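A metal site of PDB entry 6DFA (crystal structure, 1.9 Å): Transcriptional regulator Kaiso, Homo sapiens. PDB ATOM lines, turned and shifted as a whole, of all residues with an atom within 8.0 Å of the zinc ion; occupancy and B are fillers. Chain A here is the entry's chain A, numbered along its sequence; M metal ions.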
ATOM      1  N   GLN A  81     -11.901 -11.344   9.666  1.00  0.00           N
ATOM      2  CA  GLN A  81     -13.170 -12.054   9.506  1.00  0.00           C
ATOM      3  C   GLN A  81     -14.301 -11.372  10.284  1.00  0.00           C
ATOM      4  O   GLN A  81     -14.169 -11.113  11.479  1.00  0.00           O
ATOM      5  CB  GLN A  81     -13.033 -13.522   9.956  1.00  0.00           C
ATOM      6  CG  GLN A  81     -14.294 -14.365   9.595  1.00  0.00           C
ATOM      7  CD  GLN A  81     -14.156 -15.830   9.950  1.00  0.00           C
ATOM      8  OE1 GLN A  81     -13.285 -16.205  10.744  1.00  0.00           O
ATOM      9  NE2 GLN A  81     -15.014 -16.669   9.376  1.00  0.00           N
ATOM     10  N   CYS A  82     -15.391 -11.071   9.582  1.00  0.00           N
ATOM     11  CA  CYS A  82     -16.624 -10.587  10.205  1.00  0.00           C
ATOM     12  C   CYS A  82     -17.265 -11.666  11.078  1.00  0.00           C
ATOM     13  O   CYS A  82     -17.622 -12.763  10.601  1.00  0.00           O
ATOM     14  CB  CYS A  82     -17.606 -10.118   9.135  1.00  0.00           C
ATOM     15  SG  CYS A  82     -19.261  -9.657   9.778  1.00  0.00           S
ATOM     16  N   LEU A  83     -17.412 -11.366  12.364  1.00  0.00           N
ATOM     17  CA  LEU A  83     -17.988 -12.338  13.281  1.00  0.00           C
ATOM     18  C   LEU A  83     -19.506 -12.387  13.169  1.00  0.00           C
ATOM     19  O   LEU A  83     -20.124 -13.352  13.602  1.00  0.00           O
ATOM     20  CB  LEU A  83     -17.559 -12.038  14.716  1.00  0.00           C
ATOM     21  CG  LEU A  83     -16.043 -12.164  14.938  1.00  0.00           C
ATOM     22  CD1 LEU A  83     -15.648 -11.750  16.336  1.00  0.00           C
ATOM     23  CD2 LEU A  83     -15.573 -13.582  14.639  1.00  0.00           C
ATOM     24  N   ALA A  84     -20.109 -11.393  12.544  1.00  0.00           N
ATOM     25  CA  ALA A  84     -21.567 -11.389  12.381  1.00  0.00           C
ATOM     26  C   ALA A  84     -22.036 -12.403  11.321  1.00  0.00           C
ATOM     27  O   ALA A  84     -23.043 -13.091  11.517  1.00  0.00           O
ATOM     28  CB  ALA A  84     -22.055  -9.990  12.027  1.00  0.00           C
ATOM     29  N   CYS A  85     -21.298 -12.523  10.215  1.00  0.00           N
ATOM     30  CA  CYS A  85     -21.734 -13.395   9.112  1.00  0.00           C
ATOM     31  C   CYS A  85     -20.622 -14.323   8.587  1.00  0.00           C
ATOM     32  O   CYS A  85     -20.873 -15.162   7.726  1.00  0.00           O
ATOM     33  CB  CYS A  85     -22.264 -12.549   7.960  1.00  0.00           C
ATOM     34  SG  CYS A  85     -20.920 -11.750   6.994  1.00  0.00           S
ATOM     35  N   GLY A  86     -19.393 -14.185   9.071  1.00  0.00           N
ATOM     36  CA  GLY A  86     -18.319 -15.083   8.675  1.00  0.00           C
ATOM     37  C   GLY A  86     -17.467 -14.681   7.476  1.00  0.00           C
ATOM     38  O   GLY A  86     -16.407 -15.320   7.198  1.00  0.00           O
ATOM     39  N   LYS A  87     -17.885 -13.637   6.750  1.00  0.00           N
ATOM     40  CA  LYS A  87     -17.143 -13.244   5.538  1.00  0.00           C
ATOM     41  C   LYS A  87     -15.779 -12.743   5.927  1.00  0.00           C
ATOM     42  O   LYS A  87     -15.650 -12.090   6.950  1.00  0.00           O
ATOM     43  CB  LYS A  87     -17.863 -12.175   4.715  1.00  0.00           C
ATOM     44  CG  LYS A  87     -19.144 -12.686   4.040  1.00  0.00           C
ATOM     45  CD  LYS A  87     -19.574 -11.820   2.862  1.00  0.00           C
ATOM     46  CE  LYS A  87     -20.868 -12.355   2.243  1.00  0.00           C
ATOM     47  NZ  LYS A  87     -21.056 -11.956   0.823  1.00  0.00           N
ATOM     48  N   SER A  88     -14.786 -13.030   5.090  1.00  0.00           N
ATOM     49  CA  SER A  88     -13.410 -12.592   5.359  1.00  0.00           C
ATOM     50  C   SER A  88     -12.899 -11.573   4.339  1.00  0.00           C
ATOM     51  O   SER A  88     -13.335 -11.559   3.189  1.00  0.00           O
ATOM     52  CB  SER A  88     -12.493 -13.817   5.387  1.00  0.00           C
ATOM     53  OG  SER A  88     -12.986 -14.751   6.331  1.00  0.00           O
ATOM     54  N   PHE A  89     -11.937 -10.755   4.757  1.00  0.00           N
ATOM     55  CA  PHE A  89     -11.461  -9.603   3.974  1.00  0.00           C
ATOM     56  C   PHE A  89      -9.954  -9.497   4.082  1.00  0.00           C
ATOM     57  O   PHE A  89      -9.377  -9.961   5.081  1.00  0.00           O
ATOM     58  CB  PHE A  89     -12.138  -8.318   4.463  1.00  0.00           C
ATOM     59  CG  PHE A  89     -13.657  -8.439   4.498  1.00  0.00           C
ATOM     60  CD1 PHE A  89     -14.406  -8.165   3.356  1.00  0.00           C
ATOM     61  CD2 PHE A  89     -14.302  -8.898   5.633  1.00  0.00           C
ATOM     62  CE1 PHE A  89     -15.776  -8.331   3.348  1.00  0.00           C
ATOM     63  CE2 PHE A  89     -15.683  -9.059   5.643  1.00  0.00           C
ATOM     64  CZ  PHE A  89     -16.419  -8.782   4.497  1.00  0.00           C
ATOM     65  N   MET A  95     -13.041  -4.878   5.706  1.00  0.00           N
ATOM     66  CA  MET A  95     -13.806  -5.436   6.826  1.00  0.00           C
ATOM     67  C   MET A  95     -14.705  -4.348   7.423  1.00  0.00           C
ATOM     68  O   MET A  95     -15.910  -4.563   7.638  1.00  0.00           O
ATOM     69  CB  MET A  95     -12.859  -6.016   7.896  1.00  0.00           C
ATOM     70  CG  MET A  95     -13.516  -6.416   9.246  1.00  0.00           C
ATOM     71  SD  MET A  95     -13.901  -5.057  10.404  1.00  0.00           S
ATOM     72  CE  MET A  95     -12.258  -4.316  10.620  1.00  0.00           C
ATOM     73  N   HIS A  98     -17.623  -3.288   5.141  1.00  0.00           N
ATOM     74  CA  HIS A  98     -18.644  -4.346   5.192  1.00  0.00           C
ATOM     75  C   HIS A  98     -19.506  -4.299   6.443  1.00  0.00           C
ATOM     76  O   HIS A  98     -20.745  -4.374   6.378  1.00  0.00           O
ATOM     77  CB  HIS A  98     -17.963  -5.732   5.097  1.00  0.00           C
ATOM     78  CG  HIS A  98     -18.870  -6.862   5.505  1.00  0.00           C
ATOM     79  ND1 HIS A  98     -19.802  -7.411   4.647  1.00  0.00           N
ATOM     80  CD2 HIS A  98     -18.999  -7.519   6.674  1.00  0.00           C
ATOM     81  CE1 HIS A  98     -20.461  -8.366   5.273  1.00  0.00           C
ATOM     82  NE2 HIS A  98     -19.998  -8.448   6.510  1.00  0.00           N
ATOM     83  N   ILE A  99     -18.871  -4.193   7.603  1.00  0.00           N
ATOM     84  CA  ILE A  99     -19.633  -4.259   8.836  1.00  0.00           C
ATOM     85  C   ILE A  99     -20.530  -3.016   8.988  1.00  0.00           C
ATOM     86  O   ILE A  99     -21.674  -3.114   9.435  1.00  0.00           O
ATOM     87  CB  ILE A  99     -18.693  -4.429  10.046  1.00  0.00           C
ATOM     88  CG1 ILE A  99     -17.992  -5.787   9.920  1.00  0.00           C
ATOM     89  CG2 ILE A  99     -19.471  -4.336  11.339  1.00  0.00           C
ATOM     90  CD1 ILE A  99     -17.225  -6.235  11.162  1.00  0.00           C
ATOM     91  N   LYS A 100     -20.034  -1.860   8.560  1.00  0.00           N
ATOM     92  CA  LYS A 100     -20.867  -0.667   8.597  1.00  0.00           C
ATOM     93  C   LYS A 100     -22.005  -0.736   7.596  1.00  0.00           C
ATOM     94  O   LYS A 100     -23.119  -0.358   7.907  1.00  0.00           O
ATOM     95  CB  LYS A 100     -20.014   0.588   8.335  1.00  0.00           C
ATOM     96  CG  LYS A 100     -18.990   0.866   9.430  1.00  0.00           C
ATOM     97  CD  LYS A 100     -18.263   2.218   9.165  1.00  0.00           C
ATOM     98  CE  LYS A 100     -17.202   2.500  10.233  1.00  0.00           C
ATOM     99  NZ  LYS A 100     -16.391   3.737   9.946  1.00  0.00           N
ATOM    100  N   VAL A 102     -23.294  -3.490   5.791  1.00  0.00           N
ATOM    101  CA  VAL A 102     -24.162  -4.657   5.873  1.00  0.00           C
ATOM    102  C   VAL A 102     -24.774  -4.827   7.275  1.00  0.00           C
ATOM    103  O   VAL A 102     -25.940  -5.174   7.385  1.00  0.00           O
ATOM    104  CB  VAL A 102     -23.407  -5.948   5.476  1.00  0.00           C
ATOM    105  CG1 VAL A 102     -24.300  -7.175   5.661  1.00  0.00           C
ATOM    106  CG2 VAL A 102     -22.952  -5.856   4.014  1.00  0.00           C
ATOM    107  N   HIS A 103     -24.016  -4.570   8.341  1.00  0.00           N
ATOM    108  CA  HIS A 103     -24.525  -4.851   9.690  1.00  0.00           C
ATOM    109  C   HIS A 103     -24.877  -3.578  10.478  1.00  0.00           C
ATOM    110  O   HIS A 103     -25.417  -3.666  11.584  1.00  0.00           O
ATOM    111  CB  HIS A 103     -23.506  -5.699  10.452  1.00  0.00           C
ATOM    112  CG  HIS A 103     -23.202  -7.008   9.791  1.00  0.00           C
ATOM    113  ND1 HIS A 103     -24.180  -7.970   9.589  1.00  0.00           N
ATOM    114  CD2 HIS A 103     -22.052  -7.523   9.264  1.00  0.00           C
ATOM    115  CE1 HIS A 103     -23.656  -9.008   8.964  1.00  0.00           C
ATOM    116  NE2 HIS A 103     -22.372  -8.776   8.768  1.00  0.00           N
ATOM    117  N   LEU A 113     -16.314  -7.055  16.873  1.00  0.00           N
ATOM    118  CA  LEU A 113     -17.140  -7.448  15.726  1.00  0.00           C
ATOM    119  C   LEU A 113     -16.338  -8.191  14.664  1.00  0.00           C
ATOM    120  O   LEU A 113     -16.904  -8.756  13.722  1.00  0.00           O
ATOM    121  CB  LEU A 113     -17.770  -6.213  15.085  1.00  0.00           C
ATOM    122  CG  LEU A 113     -18.666  -5.430  16.065  1.00  0.00           C
ATOM    123  CD1 LEU A 113     -19.245  -4.191  15.413  1.00  0.00           C
ATOM    124  CD2 LEU A 113     -19.774  -6.323  16.609  1.00  0.00           C
HETATM  125 ZN    ZN M   1     -20.622  -9.699   8.015  1.00  0.00          ZN
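The backbone NH (N) of Ala 84 sits close to the side-chain sulfur (SG) of Cys 82 (3.4 Å).
N of Cys 82 lies within hydrogen-bond range of O of Lys 87, at 2.8 Å.
The backbone NH of Lys 87 sits close to the side-chain sulfur of Cys 85, at 3.6 Å.
The zinc ion is bound by NE2 of His 98 (2.1 Å), NE2 of His 103 (2.1 Å), SG of Cys 82 (2.2 Å) and SG of Cys 85 (2.3 Å).
The zinc ion has four donor atoms within binding distance.
Four residues have an atom within 4 Å of the zinc ion: Cys 82, Cys 85, His 98 and His 103.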
